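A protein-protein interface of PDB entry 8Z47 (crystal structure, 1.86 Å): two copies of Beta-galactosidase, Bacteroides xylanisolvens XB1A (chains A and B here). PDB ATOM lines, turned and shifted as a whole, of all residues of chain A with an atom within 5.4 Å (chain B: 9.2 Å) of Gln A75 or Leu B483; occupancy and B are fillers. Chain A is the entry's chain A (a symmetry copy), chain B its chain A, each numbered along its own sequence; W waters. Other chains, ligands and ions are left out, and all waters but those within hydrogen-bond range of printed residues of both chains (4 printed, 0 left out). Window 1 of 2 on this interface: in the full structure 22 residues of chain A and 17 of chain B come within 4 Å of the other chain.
Arg B482 touches Ser A44 (CD to O, 3.5 Å).
Ser A44 touches Leu B483 (CB to O, 3.4 Å).
CA of Leu B484 touches OG of Ser A44 (3.5 Å).
OG of Ser A47 touches CA of Arg B482, 3.2 Å away.
Thr A48 touches Ala B480 (CG2 to O, 3.9 Å).
Arg B482 touches Thr A48.
Glu A74 touches Leu B483 (OE2 to CD2, 3.8 Å).
Leu B483 touches Gln A75 (CD1 to CG, 3.7 Å).
The side-chain hydroxyl (OG) of Ser A44 lies within hydrogen-bond range of the side-chain carboxylate (OE1) of Glu B488 (2.6 Å).
OG1 of Thr A48 is in hydrogen-bond range of O of Thr B481, at 2.8 Å.
The side-chain amide nitrogen (ND2) of Asn B485 sits at hydrogen-bond distance from the side-chain carboxylate (OE2) of Glu A74 (2.9 Å).
OE1 of Glu A74 is in hydrogen-bond range of NE2 of Gln B466 (3.1 Å).
The backbone NH (N) of Leu B483 sits at hydrogen-bond distance from the side-chain hydroxyl (OG) of Ser A47 (2.9 Å).
N of Asn B485 is in hydrogen-bond range of OG of Ser A44, at 3.0 Å.
Of the 23 printed residues of chain B, 8 touch a printed residue of chain A.
Hydrophobic or aromatic side chains of chain B that line the printed part of chain A: Leu B483.
Among the printed residues, no Asp or Glu carboxylate lies within 4 Å of a Lys or Arg side-chain nitrogen of the other chain.
O of Ser A44 lies within hydrogen-bond range of OG of Ser A47.
The backbone carbonyl oxygen (O) of Glu B469 sits at hydrogen-bond distance from the backbone NH (N) of Thr B481 (2.7 Å).
The backbone NH (N) of Thr B539 lies within hydrogen-bond range of the backbone carbonyl oxygen (O) of Gln B466 (2.9 Å).
The backbone carbonyl oxygen of Val B467 is in hydrogen-bond range of the backbone NH of Leu B484 (2.9 Å).
NH2 of Arg B482 lies within salt-bridge range of OE1 of Glu B469 (2.9 Å).
NE2 of Gln A75 is in hydrogen-bond range of O of Ser A47, at 2.8 Å.
Water W3 lies within hydrogen-bond range of the side-chain carboxylate of Glu A74 (2.7 Å), the backbone carbonyl oxygen of Lys B465 (2.8 Å), the side-chain amide nitrogen of Asn B492 (2.9 Å) and the side-chain amide nitrogen of Asn B485 (3.2 Å).
Water W4 bridges OG of Ser A44 (2.8 Å) and O of Asn B485 (3.2 Å).
Water W1 bridges NH1 of Arg B482 (2.8 Å) and N of Ser A44 (3.5 Å).
Water W2 bridges the backbone carbonyl oxygen of Glu A74 (3.1 Å) and the side-chain amide nitrogen of Gln B466 (3.3 Å).
No position is printed for both chains.
Gln A75 touches one residue of chain B.
Leu B483 touches just these residues of chain A: Ser A44 (3.4 Å), Ser A47 (2.9 Å), Glu A74 (3.8 Å) and Gln A75 (3.7 Å).
Ser A47 touches just these residues of chain B: Arg B482 and Leu B483.
Ala A72 touches none of the printed residues of chain B.
Glu A74 touches three residues of chain B.
Of the printed residues of chain A, Arg B482 touches Ser A44, Ser A47 and Thr A48.
Of the printed residues of chain A, Leu B484 touches Ser A44 (3.5 Å).
Of the printed residues of chain B, Ser A44 touches Arg B482 (3.5 Å), Leu B483 (3.4 Å), Leu B484 (3.5 Å), Asn B485 (3.0 Å) and Glu B488 (2.6 Å).
Phe A76 touches none of the printed residues of chain B.
Val B467 touches none of the printed residues of chain A.
The nearest residue of chain A that does not touch Leu B483 is Thr A48 (4.7 Å).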
ATOM      1  N   SER A  44      15.015 -13.801  32.058  1.00  0.00           N
ATOM      2  CA  SER A  44      15.235 -12.936  30.913  1.00  0.00           C
ATOM      3  C   SER A  44      15.216 -11.439  31.276  1.00  0.00           C
ATOM      4  O   SER A  44      15.231 -10.587  30.377  1.00  0.00           O
ATOM      5  CB  SER A  44      14.225 -13.228  29.823  1.00  0.00           C
ATOM      6  OG  SER A  44      14.124 -14.598  29.466  1.00  0.00           O
ATOM      7  N   ALA A  46      17.383  -9.437  32.766  1.00  0.00           N
ATOM      8  CA  ALA A  46      18.597  -8.666  32.631  1.00  0.00           C
ATOM      9  C   ALA A  46      19.124  -8.764  31.203  1.00  0.00           C
ATOM     10  O   ALA A  46      20.287  -8.489  30.963  1.00  0.00           O
ATOM     11  CB  ALA A  46      19.590  -9.113  33.686  1.00  0.00           C
ATOM     12  N   SER A  47      18.246  -9.093  30.247  1.00  0.00           N
ATOM     13  CA  SER A  47      18.641  -9.297  28.865  1.00  0.00           C
ATOM     14  C   SER A  47      18.778  -7.988  28.074  1.00  0.00           C
ATOM     15  O   SER A  47      19.375  -8.046  27.015  1.00  0.00           O
ATOM     16  CB  SER A  47      17.725 -10.269  28.145  1.00  0.00           C
ATOM     17  OG  SER A  47      16.378  -9.804  28.087  1.00  0.00           O
ATOM     18  N   THR A  48      18.132  -6.876  28.490  1.00  0.00           N
ATOM     19  CA  THR A  48      18.400  -5.553  27.946  1.00  0.00           C
ATOM     20  C   THR A  48      18.588  -4.587  29.110  1.00  0.00           C
ATOM     21  O   THR A  48      18.009  -4.809  30.169  1.00  0.00           O
ATOM     22  CB  THR A  48      17.286  -5.042  27.017  1.00  0.00           C
ATOM     23  OG1 THR A  48      16.132  -4.866  27.835  1.00  0.00           O
ATOM     24  CG2 THR A  48      17.023  -5.961  25.841  1.00  0.00           C
ATOM     25  N   ALA A  72      24.579 -13.712  30.446  1.00  0.00           N
ATOM     26  CA  ALA A  72      24.418 -14.843  29.546  1.00  0.00           C
ATOM     27  C   ALA A  72      25.606 -14.846  28.588  1.00  0.00           C
ATOM     28  O   ALA A  72      25.921 -13.817  27.967  1.00  0.00           O
ATOM     29  CB  ALA A  72      23.122 -14.752  28.761  1.00  0.00           C
ATOM     30  N   TRP A  73      26.205 -16.013  28.420  1.00  0.00           N
ATOM     31  CA  TRP A  73      27.376 -16.144  27.567  1.00  0.00           C
ATOM     32  C   TRP A  73      27.018 -15.680  26.157  1.00  0.00           C
ATOM     33  O   TRP A  73      27.769 -14.936  25.506  1.00  0.00           O
ATOM     34  CB  TRP A  73      27.869 -17.588  27.634  1.00  0.00           C
ATOM     35  CG  TRP A  73      29.205 -17.891  27.000  1.00  0.00           C
ATOM     36  CD1 TRP A  73      30.115 -17.020  26.466  1.00  0.00           C
ATOM     37  CD2 TRP A  73      29.738 -19.215  26.777  1.00  0.00           C
ATOM     38  NE1 TRP A  73      31.202 -17.709  25.979  1.00  0.00           N
ATOM     39  CE2 TRP A  73      30.985 -19.049  26.125  1.00  0.00           C
ATOM     40  CE3 TRP A  73      29.293 -20.512  27.051  1.00  0.00           C
ATOM     41  CZ2 TRP A  73      31.778 -20.135  25.766  1.00  0.00           C
ATOM     42  CZ3 TRP A  73      30.057 -21.585  26.666  1.00  0.00           C
ATOM     43  CH2 TRP A  73      31.294 -21.393  26.028  1.00  0.00           C
ATOM     44  N   GLU A  74      25.847 -16.096  25.689  1.00  0.00           N
ATOM     45  CA  GLU A  74      25.478 -15.803  24.317  1.00  0.00           C
ATOM     46  C   GLU A  74      25.491 -14.292  24.066  1.00  0.00           C
ATOM     47  O   GLU A  74      25.670 -13.866  22.937  1.00  0.00           O
ATOM     48  CB  GLU A  74      24.118 -16.407  23.946  1.00  0.00           C
ATOM     49  CG  GLU A  74      22.958 -15.847  24.791  1.00  0.00           C
ATOM     50  CD  GLU A  74      21.590 -16.469  24.549  1.00  0.00           C
ATOM     51  OE1 GLU A  74      21.405 -17.029  23.450  1.00  0.00           O
ATOM     52  OE2 GLU A  74      20.709 -16.369  25.431  1.00  0.00           O
ATOM     53  N   GLN A  75      25.201 -13.473  25.092  1.00  0.00           N
ATOM     54  CA  GLN A  75      25.152 -12.038  24.929  1.00  0.00           C
ATOM     55  C   GLN A  75      26.514 -11.433  25.188  1.00  0.00           C
ATOM     56  O   GLN A  75      26.833 -10.418  24.603  1.00  0.00           O
ATOM     57  CB  GLN A  75      24.146 -11.352  25.851  1.00  0.00           C
ATOM     58  CG  GLN A  75      22.719 -11.731  25.485  1.00  0.00           C
ATOM     59  CD  GLN A  75      21.716 -11.073  26.382  1.00  0.00           C
ATOM     60  OE1 GLN A  75      21.624 -11.468  27.544  1.00  0.00           O
ATOM     61  NE2 GLN A  75      21.044 -10.044  25.864  1.00  0.00           N
ATOM     62  N   PHE A  76      27.251 -12.012  26.139  1.00  0.00           N
ATOM     63  CA  PHE A  76      28.514 -11.461  26.585  1.00  0.00           C
ATOM     64  C   PHE A  76      29.622 -11.681  25.542  1.00  0.00           C
ATOM     65  O   PHE A  76      30.439 -10.786  25.341  1.00  0.00           O
ATOM     66  CB  PHE A  76      28.897 -12.098  27.917  1.00  0.00           C
ATOM     67  CG  PHE A  76      30.227 -11.604  28.449  1.00  0.00           C
ATOM     68  CD1 PHE A  76      30.395 -10.287  28.858  1.00  0.00           C
ATOM     69  CD2 PHE A  76      31.291 -12.469  28.578  1.00  0.00           C
ATOM     70  CE1 PHE A  76      31.611  -9.860  29.374  1.00  0.00           C
ATOM     71  CE2 PHE A  76      32.499 -12.028  29.092  1.00  0.00           C
ATOM     72  CZ  PHE A  76      32.662 -10.733  29.486  1.00  0.00           C
ATOM     73  N   GLU A  77      29.664 -12.860  24.932  1.00  0.00           N
ATOM     74  CA  GLU A  77      30.640 -13.161  23.884  1.00  0.00           C
ATOM     75  C   GLU A  77      29.907 -13.579  22.612  1.00  0.00           C
ATOM     76  O   GLU A  77      29.831 -14.767  22.277  1.00  0.00           O
ATOM     77  CB  GLU A  77      31.620 -14.241  24.324  1.00  0.00           C
ATOM     78  CG  GLU A  77      32.859 -14.356  23.420  1.00  0.00           C
ATOM     79  CD  GLU A  77      33.839 -15.455  23.758  1.00  0.00           C
ATOM     80  OE1 GLU A  77      33.508 -16.307  24.609  1.00  0.00           O
ATOM     81  OE2 GLU A  77      34.946 -15.505  23.138  1.00  0.00           O
ATOM     82  N   PRO A  78      29.303 -12.616  21.882  1.00  0.00           N
ATOM     83  CA  PRO A  78      28.395 -12.942  20.791  1.00  0.00           C
ATOM     84  C   PRO A  78      29.107 -13.447  19.539  1.00  0.00           C
ATOM     85  O   PRO A  78      28.506 -14.135  18.727  1.00  0.00           O
ATOM     86  CB  PRO A  78      27.617 -11.614  20.538  1.00  0.00           C
ATOM     87  CG  PRO A  78      28.547 -10.523  21.034  1.00  0.00           C
ATOM     88  CD  PRO A  78      29.382 -11.170  22.145  1.00  0.00           C
ATOM     89  N   ASP A  84      30.960  -8.093  24.961  1.00  0.00           N
ATOM     90  CA  ASP A  84      30.056  -6.980  25.064  1.00  0.00           C
ATOM     91  C   ASP A  84      29.735  -6.733  26.538  1.00  0.00           C
ATOM     92  O   ASP A  84      29.072  -7.544  27.181  1.00  0.00           O
ATOM     93  CB  ASP A  84      28.821  -7.260  24.245  1.00  0.00           C
ATOM     94  CG  ASP A  84      27.793  -6.160  24.254  1.00  0.00           C
ATOM     95  OD1 ASP A  84      27.981  -5.186  25.021  1.00  0.00           O
ATOM     96  OD2 ASP A  84      26.816  -6.321  23.471  1.00  0.00           O
ATOM     97  N   LEU A  87      25.712  -4.999  29.353  1.00  0.00           N
ATOM     98  CA  LEU A  87      24.735  -5.452  30.346  1.00  0.00           C
ATOM     99  C   LEU A  87      25.363  -5.492  31.744  1.00  0.00           C
ATOM    100  O   LEU A  87      24.751  -4.993  32.697  1.00  0.00           O
ATOM    101  CB  LEU A  87      24.073  -6.777  29.922  1.00  0.00           C
ATOM    102  CG  LEU A  87      23.263  -6.703  28.620  1.00  0.00           C
ATOM    103  CD1 LEU A  87      22.906  -8.080  28.127  1.00  0.00           C
ATOM    104  CD2 LEU A  87      22.007  -5.831  28.735  1.00  0.00           C
ATOM    105  N   ILE B 464      15.103 -23.950  17.942  1.00  0.00           N
ATOM    106  CA  ILE B 464      15.225 -22.520  18.167  1.00  0.00           C
ATOM    107  C   ILE B 464      16.680 -22.210  18.503  1.00  0.00           C
ATOM    108  O   ILE B 464      17.274 -22.888  19.347  1.00  0.00           O
ATOM    109  CB  ILE B 464      14.298 -22.053  19.307  1.00  0.00           C
ATOM    110  CG1 ILE B 464      12.825 -22.079  18.876  1.00  0.00           C
ATOM    111  CG2 ILE B 464      14.732 -20.678  19.831  1.00  0.00           C
ATOM    112  CD1 ILE B 464      11.823 -21.990  20.011  1.00  0.00           C
ATOM    113  N   LYS B 465      17.226 -21.166  17.873  1.00  0.00           N
ATOM    114  CA  LYS B 465      18.555 -20.678  18.215  1.00  0.00           C
ATOM    115  C   LYS B 465      18.459 -19.571  19.264  1.00  0.00           C
ATOM    116  O   LYS B 465      19.080 -19.664  20.329  1.00  0.00           O
ATOM    117  CB  LYS B 465      19.293 -20.189  16.962  1.00  0.00           C
ATOM    118  CG  LYS B 465      20.821 -20.262  17.058  1.00  0.00           C
ATOM    119  CD  LYS B 465      21.624 -19.458  16.042  1.00  0.00           C
ATOM    120  CE  LYS B 465      20.951 -19.299  14.729  1.00  0.00           C
ATOM    121  NZ  LYS B 465      21.895 -18.762  13.758  1.00  0.00           N
ATOM    122  N   GLN B 466      17.746 -18.495  18.915  1.00  0.00           N
ATOM    123  CA  GLN B 466      17.484 -17.401  19.837  1.00  0.00           C
ATOM    124  C   GLN B 466      16.091 -16.781  19.634  1.00  0.00           C
ATOM    125  O   GLN B 466      15.538 -16.718  18.528  1.00  0.00           O
ATOM    126  CB  GLN B 466      18.521 -16.275  19.740  1.00  0.00           C
ATOM    127  CG  GLN B 466      19.974 -16.695  19.949  1.00  0.00           C
ATOM    128  CD  GLN B 466      20.917 -15.516  19.892  1.00  0.00           C
ATOM    129  OE1 GLN B 466      21.103 -14.909  18.834  1.00  0.00           O
ATOM    130  NE2 GLN B 466      21.547 -15.192  21.013  1.00  0.00           N
ATOM    131  N   VAL B 467      15.597 -16.164  20.713  1.00  0.00           N
ATOM    132  CA  VAL B 467      14.278 -15.529  20.719  1.00  0.00           C
ATOM    133  C   VAL B 467      14.406 -14.138  21.330  1.00  0.00           C
ATOM    134  O   VAL B 467      14.970 -13.974  22.422  1.00  0.00           O
ATOM    135  CB  VAL B 467      13.222 -16.344  21.491  1.00  0.00           C
ATOM    136  CG1 VAL B 467      11.850 -15.633  21.520  1.00  0.00           C
ATOM    137  CG2 VAL B 467      13.108 -17.762  20.960  1.00  0.00           C
ATOM    138  N   TRP B 468      13.879 -13.133  20.615  1.00  0.00           N
ATOM    139  CA  TRP B 468      13.770 -11.807  21.201  1.00  0.00           C
ATOM    140  C   TRP B 468      12.302 -11.403  21.204  1.00  0.00           C
ATOM    141  O   TRP B 468      11.561 -11.706  20.250  1.00  0.00           O
ATOM    142  CB  TRP B 468      14.596 -10.734  20.465  1.00  0.00           C
ATOM    143  CG  TRP B 468      16.089 -10.946  20.426  1.00  0.00           C
ATOM    144  CD1 TRP B 468      17.083 -10.394  21.197  1.00  0.00           C
ATOM    145  CD2 TRP B 468      16.738 -11.812  19.492  1.00  0.00           C
ATOM    146  NE1 TRP B 468      18.313 -10.862  20.796  1.00  0.00           N
ATOM    147  CE2 TRP B 468      18.123 -11.734  19.752  1.00  0.00           C
ATOM    148  CE3 TRP B 468      16.268 -12.619  18.446  1.00  0.00           C
ATOM    149  CZ2 TRP B 468      19.041 -12.464  19.000  1.00  0.00           C
ATOM    150  CZ3 TRP B 468      17.179 -13.322  17.690  1.00  0.00           C
ATOM    151  CH2 TRP B 468      18.553 -13.237  17.967  1.00  0.00           C
ATOM    152  N   GLU B 469      11.912 -10.711  22.280  1.00  0.00           N
ATOM    153  CA  GLU B 469      10.653 -10.001  22.318  1.00  0.00           C
ATOM    154  C   GLU B 469      10.921  -8.534  21.974  1.00  0.00           C
ATOM    155  O   GLU B 469      11.930  -7.969  22.392  1.00  0.00           O
ATOM    156  CB  GLU B 469      10.004 -10.096  23.700  1.00  0.00           C
ATOM    157  CG  GLU B 469       8.780  -9.184  23.828  1.00  0.00           C
ATOM    158  CD  GLU B 469       7.756  -9.376  24.933  1.00  0.00           C
ATOM    159  OE1 GLU B 469       8.110  -9.830  26.032  1.00  0.00           O
ATOM    160  OE2 GLU B 469       6.577  -8.957  24.713  1.00  0.00           O
ATOM    161  N   GLY B 470       9.995  -7.886  21.258  1.00  0.00           N
ATOM    162  CA  GLY B 470      10.144  -6.464  21.012  1.00  0.00           C
ATOM    163  C   GLY B 470       8.983  -5.881  20.196  1.00  0.00           C
ATOM    164  O   GLY B 470       7.834  -6.281  20.295  1.00  0.00           O
ATOM    165  N   TRP B 478      13.120  -2.158  14.336  1.00  0.00           N
ATOM    166  CA  TRP B 478      12.985  -3.174  15.371  1.00  0.00           C
ATOM    167  C   TRP B 478      13.786  -2.781  16.612  1.00  0.00           C
ATOM    168  O   TRP B 478      14.918  -2.342  16.493  1.00  0.00           O
ATOM    169  CB  TRP B 478      13.476  -4.527  14.831  1.00  0.00           C
ATOM    170  CG  TRP B 478      13.488  -5.641  15.853  1.00  0.00           C
ATOM    171  CD1 TRP B 478      14.588  -6.135  16.477  1.00  0.00           C
ATOM    172  CD2 TRP B 478      12.351  -6.363  16.398  1.00  0.00           C
ATOM    173  NE1 TRP B 478      14.228  -7.127  17.344  1.00  0.00           N
ATOM    174  CE2 TRP B 478      12.864  -7.284  17.334  1.00  0.00           C
ATOM    175  CE3 TRP B 478      10.963  -6.332  16.198  1.00  0.00           C
ATOM    176  CZ2 TRP B 478      12.048  -8.169  18.044  1.00  0.00           C
ATOM    177  CZ3 TRP B 478      10.157  -7.188  16.922  1.00  0.00           C
ATOM    178  CH2 TRP B 478      10.692  -8.090  17.841  1.00  0.00           C
ATOM    179  N   LYS B 479      13.159  -2.880  17.792  1.00  0.00           N
ATOM    180  CA  LYS B 479      13.796  -2.690  19.087  1.00  0.00           C
ATOM    181  C   LYS B 479      13.371  -3.858  19.985  1.00  0.00           C
ATOM    182  O   LYS B 479      12.190  -3.993  20.289  1.00  0.00           O
ATOM    183  CB  LYS B 479      13.355  -1.341  19.657  1.00  0.00           C
ATOM    184  CG  LYS B 479      13.820  -0.935  21.033  1.00  0.00           C
ATOM    185  CD  LYS B 479      15.327  -1.045  21.243  1.00  0.00           C
ATOM    186  CE  LYS B 479      15.678  -0.209  22.422  1.00  0.00           C
ATOM    187  NZ  LYS B 479      17.116  -0.147  22.643  1.00  0.00           N
ATOM    188  N   ALA B 480      14.344  -4.667  20.400  1.00  0.00           N
ATOM    189  CA  ALA B 480      14.129  -5.764  21.329  1.00  0.00           C
ATOM    190  C   ALA B 480      13.942  -5.211  22.739  1.00  0.00           C
ATOM    191  O   ALA B 480      14.695  -4.349  23.171  1.00  0.00           O
ATOM    192  CB  ALA B 480      15.308  -6.697  21.286  1.00  0.00           C
ATOM    193  N   THR B 481      12.972  -5.750  23.465  1.00  0.00           N
ATOM    194  CA  THR B 481      12.804  -5.408  24.865  1.00  0.00           C
ATOM    195  C   THR B 481      13.460  -6.467  25.772  1.00  0.00           C
ATOM    196  O   THR B 481      13.897  -6.152  26.876  1.00  0.00           O
ATOM    197  CB  THR B 481      11.337  -5.192  25.195  1.00  0.00           C
ATOM    198  OG1 THR B 481      10.556  -6.285  24.740  1.00  0.00           O
ATOM    199  CG2 THR B 481      10.823  -3.892  24.584  1.00  0.00           C
ATOM    200  N   ARG B 482      13.433  -7.726  25.346  1.00  0.00           N
ATOM    201  CA  ARG B 482      14.189  -8.776  26.034  1.00  0.00           C
ATOM    202  C   ARG B 482      14.700  -9.799  25.009  1.00  0.00           C
ATOM    203  O   ARG B 482      14.111  -9.995  23.943  1.00  0.00           O
ATOM    204  CB  ARG B 482      13.340  -9.536  27.067  1.00  0.00           C
ATOM    205  CG  ARG B 482      12.946  -8.769  28.326  1.00  0.00           C
ATOM    206  CD  ARG B 482      12.098  -9.602  29.294  1.00  0.00           C
ATOM    207  NE  ARG B 482      10.740  -9.795  28.782  1.00  0.00           N
ATOM    208  CZ  ARG B 482       9.838 -10.608  29.311  1.00  0.00           C
ATOM    209  NH1 ARG B 482      10.102 -11.309  30.416  1.00  0.00           N
ATOM    210  NH2 ARG B 482       8.665 -10.716  28.720  1.00  0.00           N
ATOM    211  N   LEU B 483      15.812 -10.450  25.354  1.00  0.00           N
ATOM    212  CA  LEU B 483      16.144 -11.761  24.821  1.00  0.00           C
ATOM    213  C   LEU B 483      15.474 -12.779  25.744  1.00  0.00           C
ATOM    214  O   LEU B 483      15.878 -12.912  26.902  1.00  0.00           O
ATOM    215  CB  LEU B 483      17.659 -11.960  24.743  1.00  0.00           C
ATOM    216  CG  LEU B 483      18.163 -13.050  23.779  1.00  0.00           C
ATOM    217  CD1 LEU B 483      19.673 -13.012  23.863  1.00  0.00           C
ATOM    218  CD2 LEU B 483      17.667 -14.463  24.104  1.00  0.00           C
ATOM    219  N   LEU B 484      14.452 -13.473  25.232  1.00  0.00           N
ATOM    220  CA  LEU B 484      13.726 -14.509  25.981  1.00  0.00           C
ATOM    221  C   LEU B 484      14.493 -15.830  25.922  1.00  0.00           C
ATOM    222  O   LEU B 484      14.894 -16.297  24.846  1.00  0.00           O
ATOM    223  CB  LEU B 484      12.307 -14.742  25.458  1.00  0.00           C
ATOM    224  CG  LEU B 484      11.333 -13.552  25.517  1.00  0.00           C
ATOM    225  CD1 LEU B 484       9.948 -13.945  25.030  1.00  0.00           C
ATOM    226  CD2 LEU B 484      11.213 -12.887  26.880  1.00  0.00           C
ATOM    227  N   ASN B 485      14.761 -16.401  27.105  1.00  0.00           N
ATOM    228  CA  ASN B 485      15.429 -17.691  27.206  1.00  0.00           C
ATOM    229  C   ASN B 485      15.046 -18.301  28.572  1.00  0.00           C
ATOM    230  O   ASN B 485      14.224 -17.749  29.304  1.00  0.00           O
ATOM    231  CB  ASN B 485      16.904 -17.479  26.862  1.00  0.00           C
ATOM    232  CG  ASN B 485      17.680 -18.744  26.567  1.00  0.00           C
ATOM    233  OD1 ASN B 485      17.249 -19.877  26.835  1.00  0.00           O
ATOM    234  ND2 ASN B 485      18.837 -18.562  25.976  1.00  0.00           N
ATOM    235  N   GLY B 486      15.649 -19.437  28.922  1.00  0.00           N
ATOM    236  CA  GLY B 486      15.334 -20.103  30.170  1.00  0.00           C
ATOM    237  C   GLY B 486      13.837 -20.387  30.299  1.00  0.00           C
ATOM    238  O   GLY B 486      13.174 -20.952  29.411  1.00  0.00           O
ATOM    239  N   ASP B 487      13.269 -19.995  31.448  1.00  0.00           N
ATOM    240  CA  ASP B 487      11.857 -20.250  31.672  1.00  0.00           C
ATOM    241  C   ASP B 487      10.996 -19.687  30.540  1.00  0.00           C
ATOM    242  O   ASP B 487       9.949 -20.247  30.209  1.00  0.00           O
ATOM    243  CB  ASP B 487      11.415 -19.661  33.005  1.00  0.00           C
ATOM    244  CG  ASP B 487      12.016 -20.265  34.270  1.00  0.00           C
ATOM    245  OD1 ASP B 487      12.536 -21.408  34.194  1.00  0.00           O
ATOM    246  OD2 ASP B 487      11.951 -19.578  35.329  1.00  0.00           O
ATOM    247  N   GLU B 488      11.427 -18.574  29.952  1.00  0.00           N
ATOM    248  CA  GLU B 488      10.575 -17.828  29.048  1.00  0.00           C
ATOM    249  C   GLU B 488      10.445 -18.533  27.696  1.00  0.00           C
ATOM    250  O   GLU B 488       9.540 -18.163  26.931  1.00  0.00           O
ATOM    251  CB  GLU B 488      11.023 -16.361  28.938  1.00  0.00           C
ATOM    252  CG  GLU B 488      10.679 -15.537  30.176  1.00  0.00           C
ATOM    253  CD  GLU B 488      11.510 -15.837  31.423  1.00  0.00           C
ATOM    254  OE1 GLU B 488      12.757 -15.742  31.329  1.00  0.00           O
ATOM    255  OE2 GLU B 488      10.914 -16.125  32.486  1.00  0.00           O
ATOM    256  N   THR B 489      11.341 -19.500  27.408  1.00  0.00           N
ATOM    257  CA  THR B 489      11.278 -20.298  26.174  1.00  0.00           C
ATOM    258  C   THR B 489      11.376 -21.810  26.447  1.00  0.00           C
ATOM    259  O   THR B 489      11.669 -22.590  25.521  1.00  0.00           O
ATOM    260  CB  THR B 489      12.358 -19.916  25.147  1.00  0.00           C
ATOM    261  OG1 THR B 489      13.641 -20.114  25.749  1.00  0.00           O
ATOM    262  CG2 THR B 489      12.255 -18.485  24.631  1.00  0.00           C
ATOM    263  N   ASN B 492      14.636 -22.854  25.091  1.00  0.00           N
ATOM    264  CA  ASN B 492      14.557 -22.859  23.644  1.00  0.00           C
ATOM    265  C   ASN B 492      13.862 -24.103  23.109  1.00  0.00           C
ATOM    266  O   ASN B 492      14.006 -24.407  21.928  1.00  0.00           O
ATOM    267  CB  ASN B 492      15.885 -22.531  22.987  1.00  0.00           C
ATOM    268  CG  ASN B 492      16.352 -21.115  23.229  1.00  0.00           C
ATOM    269  OD1 ASN B 492      15.599 -20.235  23.681  1.00  0.00           O
ATOM    270  ND2 ASN B 492      17.623 -20.876  22.956  1.00  0.00           N
ATOM    271  N   TYR B 536       7.585 -11.317  18.450  1.00  0.00           N
ATOM    272  CA  TYR B 536       8.720 -12.150  18.802  1.00  0.00           C
ATOM    273  C   TYR B 536       9.517 -12.443  17.544  1.00  0.00           C
ATOM    274  O   TYR B 536       8.948 -12.877  16.560  1.00  0.00           O
ATOM    275  CB  TYR B 536       8.184 -13.467  19.374  1.00  0.00           C
ATOM    276  CG  TYR B 536       7.299 -13.212  20.601  1.00  0.00           C
ATOM    277  CD1 TYR B 536       7.869 -12.950  21.849  1.00  0.00           C
ATOM    278  CD2 TYR B 536       5.929 -13.071  20.470  1.00  0.00           C
ATOM    279  CE1 TYR B 536       7.096 -12.689  22.967  1.00  0.00           C
ATOM    280  CE2 TYR B 536       5.147 -12.787  21.579  1.00  0.00           C
ATOM    281  CZ  TYR B 536       5.730 -12.575  22.826  1.00  0.00           C
ATOM    282  OH  TYR B 536       4.966 -12.263  23.930  1.00  0.00           O
ATOM    283  N   ARG B 537      10.817 -12.191  17.595  1.00  0.00           N
ATOM    284  CA  ARG B 537      11.733 -12.540  16.528  1.00  0.00           C
ATOM    285  C   ARG B 537      12.429 -13.839  16.905  1.00  0.00           C
ATOM    286  O   ARG B 537      13.018 -13.895  17.984  1.00  0.00           O
ATOM    287  CB  ARG B 537      12.708 -11.379  16.346  1.00  0.00           C
ATOM    288  CG  ARG B 537      13.829 -11.763  15.393  1.00  0.00           C
ATOM    289  CD  ARG B 537      14.842 -10.634  15.260  1.00  0.00           C
ATOM    290  NE  ARG B 537      16.003 -11.188  14.551  1.00  0.00           N
ATOM    291  CZ  ARG B 537      17.293 -11.020  14.843  1.00  0.00           C
ATOM    292  NH1 ARG B 537      17.674 -10.363  15.931  1.00  0.00           N
ATOM    293  NH2 ARG B 537      18.197 -11.511  14.009  1.00  0.00           N
ATOM    294  N   THR B 539      15.093 -16.842  15.699  1.00  0.00           N
ATOM    295  CA  THR B 539      16.073 -17.465  14.823  1.00  0.00           C
ATOM    296  C   THR B 539      16.113 -18.943  15.151  1.00  0.00           C
ATOM    297  O   THR B 539      15.942 -19.332  16.308  1.00  0.00           O
ATOM    298  CB  THR B 539      17.449 -16.810  14.926  1.00  0.00           C
ATOM    299  OG1 THR B 539      17.861 -16.778  16.289  1.00  0.00           O
ATOM    300  CG2 THR B 539      17.442 -15.378  14.434  1.00  0.00           C
HETATM  301  O   HOH W   1      12.064 -12.010  32.336  1.00  0.00           O
HETATM  302  O   HOH W   2      23.282 -12.494  21.564  1.00  0.00           O
HETATM  303  O   HOH W   3      19.105 -18.388  22.842  1.00  0.00           O
HETATM  304  O   HOH W   4      16.663 -15.764  29.823  1.00  0.00           O
